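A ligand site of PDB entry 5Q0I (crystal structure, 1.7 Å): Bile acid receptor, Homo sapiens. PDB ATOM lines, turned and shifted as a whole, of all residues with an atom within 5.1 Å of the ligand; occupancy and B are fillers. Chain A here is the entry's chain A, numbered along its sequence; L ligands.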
ATOM      1  N   MET A  26     -11.887  11.922  15.745  1.00  0.00           N
ATOM      2  CA  MET A  26     -11.647  13.131  14.939  1.00  0.00           C
ATOM      3  C   MET A  26     -12.915  13.355  14.114  1.00  0.00           C
ATOM      4  O   MET A  26     -13.340  12.443  13.397  1.00  0.00           O
ATOM      5  CB  MET A  26     -10.429  12.961  14.017  1.00  0.00           C
ATOM      6  CG  MET A  26     -10.168  14.206  13.162  1.00  0.00           C
ATOM      7  SD  MET A  26      -8.771  14.019  12.022  1.00  0.00           S
ATOM      8  CE  MET A  26      -7.388  14.283  13.146  1.00  0.00           C
ATOM      9  N   THR A  31     -12.277  16.167   8.067  1.00  0.00           N
ATOM     10  CA  THR A  31     -11.719  15.448   6.920  1.00  0.00           C
ATOM     11  C   THR A  31     -12.582  15.637   5.666  1.00  0.00           C
ATOM     12  O   THR A  31     -12.034  15.730   4.575  1.00  0.00           O
ATOM     13  CB  THR A  31     -11.426  13.964   7.238  1.00  0.00           C
ATOM     14  OG1 THR A  31     -12.618  13.343   7.708  1.00  0.00           O
ATOM     15  CG2 THR A  31     -10.316  13.792   8.261  1.00  0.00           C
ATOM     16  N   ILE A  34     -11.898  18.689   3.173  1.00  0.00           N
ATOM     17  CA  ILE A  34     -10.808  18.512   2.215  1.00  0.00           C
ATOM     18  C   ILE A  34     -11.329  18.146   0.813  1.00  0.00           C
ATOM     19  O   ILE A  34     -10.842  18.710  -0.172  1.00  0.00           O
ATOM     20  CB  ILE A  34      -9.738  17.528   2.737  1.00  0.00           C
ATOM     21  CG1 ILE A  34      -9.154  18.066   4.065  1.00  0.00           C
ATOM     22  CG2 ILE A  34      -8.619  17.288   1.686  1.00  0.00           C
ATOM     23  CD1 ILE A  34      -8.230  17.085   4.783  1.00  0.00           C
ATOM     24  N   PHE A  39      -9.581  23.543  -1.777  1.00  0.00           N
ATOM     25  CA  PHE A  39      -8.426  23.167  -0.984  1.00  0.00           C
ATOM     26  C   PHE A  39      -7.102  23.650  -1.590  1.00  0.00           C
ATOM     27  O   PHE A  39      -6.372  22.878  -2.206  1.00  0.00           O
ATOM     28  CB  PHE A  39      -8.426  21.657  -0.718  1.00  0.00           C
ATOM     29  CG  PHE A  39      -7.508  21.175   0.383  1.00  0.00           C
ATOM     30  CD1 PHE A  39      -7.852  21.349   1.714  1.00  0.00           C
ATOM     31  CD2 PHE A  39      -6.336  20.490   0.090  1.00  0.00           C
ATOM     32  CE1 PHE A  39      -7.040  20.853   2.743  1.00  0.00           C
ATOM     33  CE2 PHE A  39      -5.505  20.017   1.120  1.00  0.00           C
ATOM     34  CZ  PHE A  39      -5.870  20.210   2.437  1.00  0.00           C
ATOM     35  N   ASN A  44      -5.614  24.483   3.263  1.00  0.00           N
ATOM     36  CA  ASN A  44      -4.755  23.417   3.761  1.00  0.00           C
ATOM     37  C   ASN A  44      -4.183  23.833   5.129  1.00  0.00           C
ATOM     38  O   ASN A  44      -4.211  23.032   6.064  1.00  0.00           O
ATOM     39  CB  ASN A  44      -3.634  23.069   2.765  1.00  0.00           C
ATOM     40  CG  ASN A  44      -2.913  21.758   3.018  1.00  0.00           C
ATOM     41  OD1 ASN A  44      -2.316  21.159   2.107  1.00  0.00           O
ATOM     42  ND2 ASN A  44      -2.896  21.269   4.255  1.00  0.00           N
ATOM     43  N   ILE A  47      -7.232  23.917   7.791  1.00  0.00           N
ATOM     44  CA  ILE A  47      -7.682  22.556   8.127  1.00  0.00           C
ATOM     45  C   ILE A  47      -6.617  21.846   8.978  1.00  0.00           C
ATOM     46  O   ILE A  47      -6.983  21.151   9.941  1.00  0.00           O
ATOM     47  CB  ILE A  47      -8.116  21.769   6.874  1.00  0.00           C
ATOM     48  CG1 ILE A  47      -9.453  22.376   6.331  1.00  0.00           C
ATOM     49  CG2 ILE A  47      -8.261  20.252   7.174  1.00  0.00           C
ATOM     50  CD1 ILE A  47      -9.825  21.987   4.915  1.00  0.00           C
ATOM     51  N   LEU A  48      -5.323  22.073   8.665  1.00  0.00           N
ATOM     52  CA  LEU A  48      -4.199  21.552   9.442  1.00  0.00           C
ATOM     53  C   LEU A  48      -4.360  22.015  10.912  1.00  0.00           C
ATOM     54  O   LEU A  48      -4.227  21.196  11.826  1.00  0.00           O
ATOM     55  CB  LEU A  48      -2.864  22.092   8.836  1.00  0.00           C
ATOM     56  CG  LEU A  48      -1.489  21.755   9.462  1.00  0.00           C
ATOM     57  CD1 LEU A  48      -1.122  22.694  10.597  1.00  0.00           C
ATOM     58  CD2 LEU A  48      -1.379  20.306   9.885  1.00  0.00           C
ATOM     59  N   MET A  51      -7.255  20.258  12.676  1.00  0.00           N
ATOM     60  CA  MET A  51      -6.883  18.877  12.975  1.00  0.00           C
ATOM     61  C   MET A  51      -5.899  18.786  14.104  1.00  0.00           C
ATOM     62  O   MET A  51      -6.048  17.932  14.980  1.00  0.00           O
ATOM     63  CB  MET A  51      -6.288  18.169  11.737  1.00  0.00           C
ATOM     64  CG  MET A  51      -7.306  17.905  10.679  1.00  0.00           C
ATOM     65  SD  MET A  51      -6.595  16.887   9.373  1.00  0.00           S
ATOM     66  CE  MET A  51      -8.060  16.624   8.412  1.00  0.00           C
ATOM     67  N   ALA A  52      -4.861  19.647  14.082  1.00  0.00           N
ATOM     68  CA  ALA A  52      -3.836  19.681  15.121  1.00  0.00           C
ATOM     69  C   ALA A  52      -4.508  20.059  16.453  1.00  0.00           C
ATOM     70  O   ALA A  52      -4.205  19.460  17.471  1.00  0.00           O
ATOM     71  CB  ALA A  52      -2.765  20.680  14.769  1.00  0.00           C
ATOM     72  N   HIS A  55      -6.101  17.033  17.816  1.00  0.00           N
ATOM     73  CA  HIS A  55      -5.083  16.172  18.403  1.00  0.00           C
ATOM     74  C   HIS A  55      -4.709  16.639  19.799  1.00  0.00           C
ATOM     75  O   HIS A  55      -4.573  15.803  20.684  1.00  0.00           O
ATOM     76  CB  HIS A  55      -3.799  16.155  17.562  1.00  0.00           C
ATOM     77  CG  HIS A  55      -3.861  15.312  16.332  1.00  0.00           C
ATOM     78  ND1 HIS A  55      -4.422  14.052  16.350  1.00  0.00           N
ATOM     79  CD2 HIS A  55      -3.357  15.551  15.101  1.00  0.00           C
ATOM     80  CE1 HIS A  55      -4.297  13.589  15.120  1.00  0.00           C
ATOM     81  NE2 HIS A  55      -3.665  14.461  14.332  1.00  0.00           N
ATOM     82  N   VAL A  86       4.530  15.995  19.020  1.00  0.00           N
ATOM     83  CA  VAL A  86       4.650  15.724  17.581  1.00  0.00           C
ATOM     84  C   VAL A  86       4.557  14.229  17.273  1.00  0.00           C
ATOM     85  O   VAL A  86       3.809  13.822  16.371  1.00  0.00           O
ATOM     86  CB  VAL A  86       5.940  16.394  17.027  1.00  0.00           C
ATOM     87  CG1 VAL A  86       6.253  15.946  15.593  1.00  0.00           C
ATOM     88  CG2 VAL A  86       5.835  17.920  17.121  1.00  0.00           C
ATOM     89  N   MET A  89       1.031  12.919  17.951  1.00  0.00           N
ATOM     90  CA  MET A  89       0.146  13.385  16.871  1.00  0.00           C
ATOM     91  C   MET A  89       0.283  12.557  15.600  1.00  0.00           C
ATOM     92  O   MET A  89      -0.738  12.101  15.056  1.00  0.00           O
ATOM     93  CB  MET A  89       0.370  14.875  16.564  1.00  0.00           C
ATOM     94  CG  MET A  89      -0.136  15.774  17.664  1.00  0.00           C
ATOM     95  SD  MET A  89       0.227  17.501  17.255  1.00  0.00           S
ATOM     96  CE  MET A  89      -0.154  18.207  18.714  1.00  0.00           C
ATOM     97  N   PHE A  90       1.515  12.313  15.130  1.00  0.00           N
ATOM     98  CA  PHE A  90       1.697  11.482  13.951  1.00  0.00           C
ATOM     99  C   PHE A  90       1.219  10.056  14.137  1.00  0.00           C
ATOM    100  O   PHE A  90       0.676   9.475  13.191  1.00  0.00           O
ATOM    101  CB  PHE A  90       3.135  11.511  13.437  1.00  0.00           C
ATOM    102  CG  PHE A  90       3.478  12.774  12.689  1.00  0.00           C
ATOM    103  CD1 PHE A  90       2.809  13.111  11.516  1.00  0.00           C
ATOM    104  CD2 PHE A  90       4.500  13.601  13.126  1.00  0.00           C
ATOM    105  CE1 PHE A  90       3.132  14.286  10.808  1.00  0.00           C
ATOM    106  CE2 PHE A  90       4.845  14.758  12.404  1.00  0.00           C
ATOM    107  CZ  PHE A  90       4.158  15.096  11.259  1.00  0.00           C
ATOM    108  N   SER A  93      -2.590  10.237  13.840  1.00  0.00           N
ATOM    109  CA  SER A  93      -2.908  10.488  12.428  1.00  0.00           C
ATOM    110  C   SER A  93      -2.698   9.231  11.582  1.00  0.00           C
ATOM    111  O   SER A  93      -3.553   8.915  10.751  1.00  0.00           O
ATOM    112  CB  SER A  93      -2.072  11.627  11.878  1.00  0.00           C
ATOM    113  OG  SER A  93      -2.570  12.822  12.446  1.00  0.00           O
ATOM    114  N   ILE A  96      -5.675   6.912  12.120  1.00  0.00           N
ATOM    115  CA  ILE A  96      -6.851   7.437  11.399  1.00  0.00           C
ATOM    116  C   ILE A  96      -6.716   7.195   9.897  1.00  0.00           C
ATOM    117  O   ILE A  96      -7.599   6.596   9.266  1.00  0.00           O
ATOM    118  CB  ILE A  96      -7.136   8.914  11.739  1.00  0.00           C
ATOM    119  CG1 ILE A  96      -7.486   9.091  13.232  1.00  0.00           C
ATOM    120  CG2 ILE A  96      -8.235   9.509  10.822  1.00  0.00           C
ATOM    121  CD1 ILE A  96      -7.300  10.530  13.702  1.00  0.00           C
ATOM    122  N   PHE A  97      -5.576   7.625   9.338  1.00  0.00           N
ATOM    123  CA  PHE A  97      -5.261   7.516   7.917  1.00  0.00           C
ATOM    124  C   PHE A  97      -5.313   6.082   7.420  1.00  0.00           C
ATOM    125  O   PHE A  97      -5.919   5.820   6.394  1.00  0.00           O
ATOM    126  CB  PHE A  97      -3.874   8.124   7.646  1.00  0.00           C
ATOM    127  CG  PHE A  97      -3.520   8.233   6.200  1.00  0.00           C
ATOM    128  CD1 PHE A  97      -3.984   9.294   5.429  1.00  0.00           C
ATOM    129  CD2 PHE A  97      -2.697   7.275   5.589  1.00  0.00           C
ATOM    130  CE1 PHE A  97      -3.661   9.389   4.067  1.00  0.00           C
ATOM    131  CE2 PHE A  97      -2.355   7.392   4.242  1.00  0.00           C
ATOM    132  CZ  PHE A  97      -2.825   8.446   3.485  1.00  0.00           C
ATOM    133  N   LEU A 101     -10.529   5.769   7.841  1.00  0.00           N
ATOM    134  CA  LEU A 101     -11.166   6.459   6.710  1.00  0.00           C
ATOM    135  C   LEU A 101     -12.001   5.494   5.854  1.00  0.00           C
ATOM    136  O   LEU A 101     -11.629   4.333   5.732  1.00  0.00           O
ATOM    137  CB  LEU A 101     -10.121   7.162   5.822  1.00  0.00           C
ATOM    138  CG  LEU A 101      -9.246   8.229   6.503  1.00  0.00           C
ATOM    139  CD1 LEU A 101      -8.117   8.649   5.590  1.00  0.00           C
ATOM    140  CD2 LEU A 101     -10.066   9.452   6.906  1.00  0.00           C
ATOM    141  N   LEU A 109      -7.218  11.978   0.076  1.00  0.00           N
ATOM    142  CA  LEU A 109      -6.743  13.000   1.029  1.00  0.00           C
ATOM    143  C   LEU A 109      -5.273  13.324   0.761  1.00  0.00           C
ATOM    144  O   LEU A 109      -4.899  14.508   0.690  1.00  0.00           O
ATOM    145  CB  LEU A 109      -7.012  12.566   2.477  1.00  0.00           C
ATOM    146  CG  LEU A 109      -8.490  12.416   2.925  1.00  0.00           C
ATOM    147  CD1 LEU A 109      -8.574  12.153   4.405  1.00  0.00           C
ATOM    148  CD2 LEU A 109      -9.290  13.689   2.664  1.00  0.00           C
ATOM    149  N   ILE A 113      -3.701  17.052  -0.514  1.00  0.00           N
ATOM    150  CA  ILE A 113      -2.610  17.708   0.197  1.00  0.00           C
ATOM    151  C   ILE A 113      -1.428  17.964  -0.739  1.00  0.00           C
ATOM    152  O   ILE A 113      -0.860  19.058  -0.718  1.00  0.00           O
ATOM    153  CB  ILE A 113      -2.237  16.938   1.488  1.00  0.00           C
ATOM    154  CG1 ILE A 113      -3.408  17.064   2.515  1.00  0.00           C
ATOM    155  CG2 ILE A 113      -0.931  17.476   2.099  1.00  0.00           C
ATOM    156  CD1 ILE A 113      -3.394  16.106   3.596  1.00  0.00           C
ATOM    157  N   ILE A 118       1.275  23.779  -0.785  1.00  0.00           N
ATOM    158  CA  ILE A 118       2.224  23.691   0.344  1.00  0.00           C
ATOM    159  C   ILE A 118       3.444  22.836  -0.072  1.00  0.00           C
ATOM    160  O   ILE A 118       3.260  21.835  -0.761  1.00  0.00           O
ATOM    161  CB  ILE A 118       1.534  23.148   1.640  1.00  0.00           C
ATOM    162  CG1 ILE A 118       0.570  24.201   2.251  1.00  0.00           C
ATOM    163  CG2 ILE A 118       2.552  22.621   2.677  1.00  0.00           C
ATOM    164  CD1 ILE A 118      -0.039  23.851   3.628  1.00  0.00           C
ATOM    165  N   ILE A 123       6.068  16.614   3.509  1.00  0.00           N
ATOM    166  CA  ILE A 123       4.840  15.882   3.207  1.00  0.00           C
ATOM    167  C   ILE A 123       5.158  14.444   2.783  1.00  0.00           C
ATOM    168  O   ILE A 123       4.538  13.502   3.301  1.00  0.00           O
ATOM    169  CB  ILE A 123       3.963  16.671   2.195  1.00  0.00           C
ATOM    170  CG1 ILE A 123       3.233  17.823   2.923  1.00  0.00           C
ATOM    171  CG2 ILE A 123       2.970  15.761   1.425  1.00  0.00           C
ATOM    172  CD1 ILE A 123       2.653  18.936   1.976  1.00  0.00           C
ATOM    173  N   MET A 126       6.084  12.124   5.630  1.00  0.00           N
ATOM    174  CA  MET A 126       4.902  11.869   6.481  1.00  0.00           C
ATOM    175  C   MET A 126       4.064  10.703   5.877  1.00  0.00           C
ATOM    176  O   MET A 126       3.788   9.725   6.567  1.00  0.00           O
ATOM    177  CB  MET A 126       4.054  13.148   6.645  1.00  0.00           C
ATOM    178  CG  MET A 126       2.760  12.938   7.397  1.00  0.00           C
ATOM    179  SD  MET A 126       1.673  14.385   7.455  1.00  0.00           S
ATOM    180  CE  MET A 126       0.945  14.387   5.817  1.00  0.00           C
ATOM    181  N   PHE A 127       3.679  10.798   4.596  1.00  0.00           N
ATOM    182  CA  PHE A 127       2.932   9.739   3.924  1.00  0.00           C
ATOM    183  C   PHE A 127       3.732   8.447   3.817  1.00  0.00           C
ATOM    184  O   PHE A 127       3.165   7.373   4.036  1.00  0.00           O
ATOM    185  CB  PHE A 127       2.386  10.211   2.577  1.00  0.00           C
ATOM    186  CG  PHE A 127       1.262  11.213   2.721  1.00  0.00           C
ATOM    187  CD1 PHE A 127       1.380  12.494   2.197  1.00  0.00           C
ATOM    188  CD2 PHE A 127       0.084  10.867   3.365  1.00  0.00           C
ATOM    189  CE1 PHE A 127       0.330  13.408   2.311  1.00  0.00           C
ATOM    190  CE2 PHE A 127      -0.954  11.795   3.508  1.00  0.00           C
ATOM    191  CZ  PHE A 127      -0.820  13.063   2.977  1.00  0.00           C
ATOM    192  N   TYR A 130       3.377   6.769   7.140  1.00  0.00           N
ATOM    193  CA  TYR A 130       2.057   6.121   7.248  1.00  0.00           C
ATOM    194  C   TYR A 130       2.044   4.789   6.520  1.00  0.00           C
ATOM    195  O   TYR A 130       1.542   3.798   7.060  1.00  0.00           O
ATOM    196  CB  TYR A 130       0.933   7.020   6.711  1.00  0.00           C
ATOM    197  CG  TYR A 130       0.732   8.310   7.473  1.00  0.00           C
ATOM    198  CD1 TYR A 130       1.251   8.469   8.766  1.00  0.00           C
ATOM    199  CD2 TYR A 130       0.071   9.378   6.899  1.00  0.00           C
ATOM    200  CE1 TYR A 130       1.100   9.665   9.456  1.00  0.00           C
ATOM    201  CE2 TYR A 130      -0.146  10.552   7.609  1.00  0.00           C
ATOM    202  CZ  TYR A 130       0.377  10.695   8.888  1.00  0.00           C
ATOM    203  OH  TYR A 130       0.205  11.856   9.570  1.00  0.00           O
ATOM    204  N   MET A 211       9.613  21.922   9.967  1.00  0.00           N
ATOM    205  CA  MET A 211       8.472  21.294   9.299  1.00  0.00           C
ATOM    206  C   MET A 211       7.269  22.248   9.356  1.00  0.00           C
ATOM    207  O   MET A 211       6.694  22.554   8.304  1.00  0.00           O
ATOM    208  CB  MET A 211       8.144  19.953   9.969  1.00  0.00           C
ATOM    209  CG  MET A 211       6.886  19.317   9.470  1.00  0.00           C
ATOM    210  SD  MET A 211       6.586  17.789  10.349  1.00  0.00           S
ATOM    211  CE  MET A 211       6.104  18.407  11.940  1.00  0.00           C
ATOM    212  N   TRP A 215       4.982  24.657   6.488  1.00  0.00           N
ATOM    213  CA  TRP A 215       3.525  24.568   6.321  1.00  0.00           C
ATOM    214  C   TRP A 215       2.827  25.902   6.536  1.00  0.00           C
ATOM    215  O   TRP A 215       1.625  26.003   6.318  1.00  0.00           O
ATOM    216  CB  TRP A 215       2.939  23.444   7.205  1.00  0.00           C
ATOM    217  CG  TRP A 215       3.454  22.072   6.861  1.00  0.00           C
ATOM    218  CD1 TRP A 215       4.149  21.697   5.756  1.00  0.00           C
ATOM    219  CD2 TRP A 215       3.285  20.882   7.654  1.00  0.00           C
ATOM    220  NE1 TRP A 215       4.451  20.355   5.807  1.00  0.00           N
ATOM    221  CE2 TRP A 215       3.907  19.821   6.955  1.00  0.00           C
ATOM    222  CE3 TRP A 215       2.661  20.601   8.876  1.00  0.00           C
ATOM    223  CZ2 TRP A 215       3.920  18.508   7.429  1.00  0.00           C
ATOM    224  CZ3 TRP A 215       2.685  19.290   9.358  1.00  0.00           C
ATOM    225  CH2 TRP A 215       3.311  18.267   8.638  1.00  0.00           C
ATOM    226  N   TRP A 230       3.823  23.252  20.673  1.00  0.00           N
ATOM    227  CA  TRP A 230       4.911  23.050  19.715  1.00  0.00           C
ATOM    228  C   TRP A 230       6.118  23.987  19.900  1.00  0.00           C
ATOM    229  O   TRP A 230       7.077  23.852  19.140  1.00  0.00           O
ATOM    230  CB  TRP A 230       4.384  23.231  18.286  1.00  0.00           C
ATOM    231  CG  TRP A 230       3.510  22.120  17.774  1.00  0.00           C
ATOM    232  CD1 TRP A 230       3.557  20.794  18.100  1.00  0.00           C
ATOM    233  CD2 TRP A 230       2.535  22.242  16.745  1.00  0.00           C
ATOM    234  NE1 TRP A 230       2.624  20.094  17.369  1.00  0.00           N
ATOM    235  CE2 TRP A 230       1.985  20.964  16.530  1.00  0.00           C
ATOM    236  CE3 TRP A 230       2.044  23.326  15.995  1.00  0.00           C
ATOM    237  CZ2 TRP A 230       0.994  20.730  15.572  1.00  0.00           C
ATOM    238  CZ3 TRP A 230       1.058  23.099  15.052  1.00  0.00           C
ATOM    239  CH2 TRP A 230       0.554  21.809  14.837  1.00  0.00           C
HETATM  240  O1  LIG L   1      -3.153  17.863  11.023  1.00  0.00           O
HETATM  241  S1  LIG L   1      -2.550  16.589  11.219  1.00  0.00           S
HETATM  242  O2  LIG L   1      -3.291  15.525  11.834  1.00  0.00           O
HETATM  243  C1  LIG L   1      -1.026  16.803  12.088  1.00  0.00           C
HETATM  244  C2  LIG L   1      -0.558  18.083  12.352  1.00  0.00           C
HETATM  245  C3  LIG L   1       0.649  18.245  13.013  1.00  0.00           C
HETATM  246  C4  LIG L   1       1.402  17.154  13.431  1.00  0.00           C
HETATM  247  C5  LIG L   1       2.698  17.343  14.157  1.00  0.00           C
HETATM  248  C6  LIG L   1       0.911  15.881  13.146  1.00  0.00           C
HETATM  249  C7  LIG L   1      -0.286  15.697  12.478  1.00  0.00           C
HETATM  250  N1  LIG L   1      -2.027  16.027   9.707  1.00  0.00           N
HETATM  251  C8  LIG L   1      -1.769  14.582   9.551  1.00  0.00           C
HETATM  252  C9  LIG L   1      -2.638  13.577   8.808  1.00  0.00           C
HETATM  253  N2  LIG L   1      -3.907  13.882   8.565  1.00  0.00           N
HETATM  254  C10 LIG L   1      -4.798  12.949   7.858  1.00  0.00           C
HETATM  255  C11 LIG L   1      -6.066  12.649   8.687  1.00  0.00           C
HETATM  256  C12 LIG L   1      -5.733  12.318  10.147  1.00  0.00           C
HETATM  257  C13 LIG L   1      -6.900  11.520   8.062  1.00  0.00           C
HETATM  258  C14 LIG L   1      -5.045  13.325   6.335  1.00  0.00           C
HETATM  259  C15 LIG L   1      -5.727  14.681   6.154  1.00  0.00           C
HETATM  260  C16 LIG L   1      -3.781  13.219   5.507  1.00  0.00           C
HETATM  261  O3  LIG L   1      -2.128  12.514   8.462  1.00  0.00           O
HETATM  262  C17 LIG L   1      -1.794  16.905   8.584  1.00  0.00           C
HETATM  263  C18 LIG L   1      -0.473  17.241   8.265  1.00  0.00           C
HETATM  264  C19 LIG L   1      -0.186  18.072   7.212  1.00  0.00           C
HETATM  265  C20 LIG L   1      -2.842  17.428   7.808  1.00  0.00           C
HETATM  266  C21 LIG L   1      -2.548  18.279   6.734  1.00  0.00           C
HETATM  267  O4  LIG L   1      -3.487  18.853   5.895  1.00  0.00           O
HETATM  268  C22 LIG L   1      -4.655  19.409   6.470  1.00  0.00           C
HETATM  269  C23 LIG L   1      -1.211  18.600   6.436  1.00  0.00           C
HETATM  270  O5  LIG L   1      -1.017  19.432   5.369  1.00  0.00           O
HETATM  271  C24 LIG L   1       0.219  20.165   5.311  1.00  0.00           C
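O3 of the ligand is in hydrogen-bond range of OH of Tyr 130, at 2.7 Å. A ring nitrogen (NE2) of His 55 is in hydrogen-bond range of an oxygen (O2) of the ligand (2.7 Å). O5 of the ligand is in hydrogen-bond range of ND2 of Asn 44 (2.9 Å). The side-chain hydroxyl (OG) of Ser 93 lies within hydrogen-bond range of an oxygen (O2) of the ligand, at 2.9 Å.
The side-chain hydroxyl (OH) of Tyr 130 sits close to the side-chain sulfur (SD) of Met 126 (3.6 Å). The side-chain hydroxyl (OG) of Ser 93 sits at hydrogen-bond distance from a ring nitrogen (NE2) of His 55 (2.7 Å). The side-chain hydroxyl (OG) of Ser 93 sits at hydrogen-bond distance from the backbone carbonyl oxygen (O) of Met 89 (3.3 Å). NE1 of Trp 230 lies within hydrogen-bond range of SD of Met 89 (3.5 Å). O of Ile 96 lies within hydrogen-bond range of N of Leu 101 (3.4 Å).
Met 26 touches the ligand. Ile 34 touches the ligand. Ile 47 touches the ligand (CG2 to C22, 3.8 Å). CD2 of Leu 48 touches O1 of the ligand, 3.2 Å away. Met 51 touches the ligand (CB to O1, 3.2 Å). Ala 52 touches the ligand (N to O1, 3.9 Å). Met 89 touches the ligand (CB to C6, 3.6 Å). Phe 90 touches the ligand. Ile 96 touches the ligand (CG2 to C13, 3.7 Å). Phe 97 touches the ligand. Leu 101 touches the ligand. Ile 113 touches the ligand. Met 126 touches the ligand (SD to C18, 3.7 Å). Phe 127 touches the ligand (CE2 to C16, 3.7 Å). Trp 215 touches the ligand. Trp 230 touches the ligand. 20 residues have an atom within 4 Å of the ligand: Met 26, Ile 34, Asn 44, Ile 47, Leu 48, Met 51, Ala 52, His 55, Met 89, Phe 90, Ser 93, Ile 96, Phe 97, Leu 101, Ile 113, Met 126, Phe 127, Tyr 130, Trp 215 and Trp 230. The nearest printed residue that does not touch the ligand is Ile 118 (4.1 Å).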
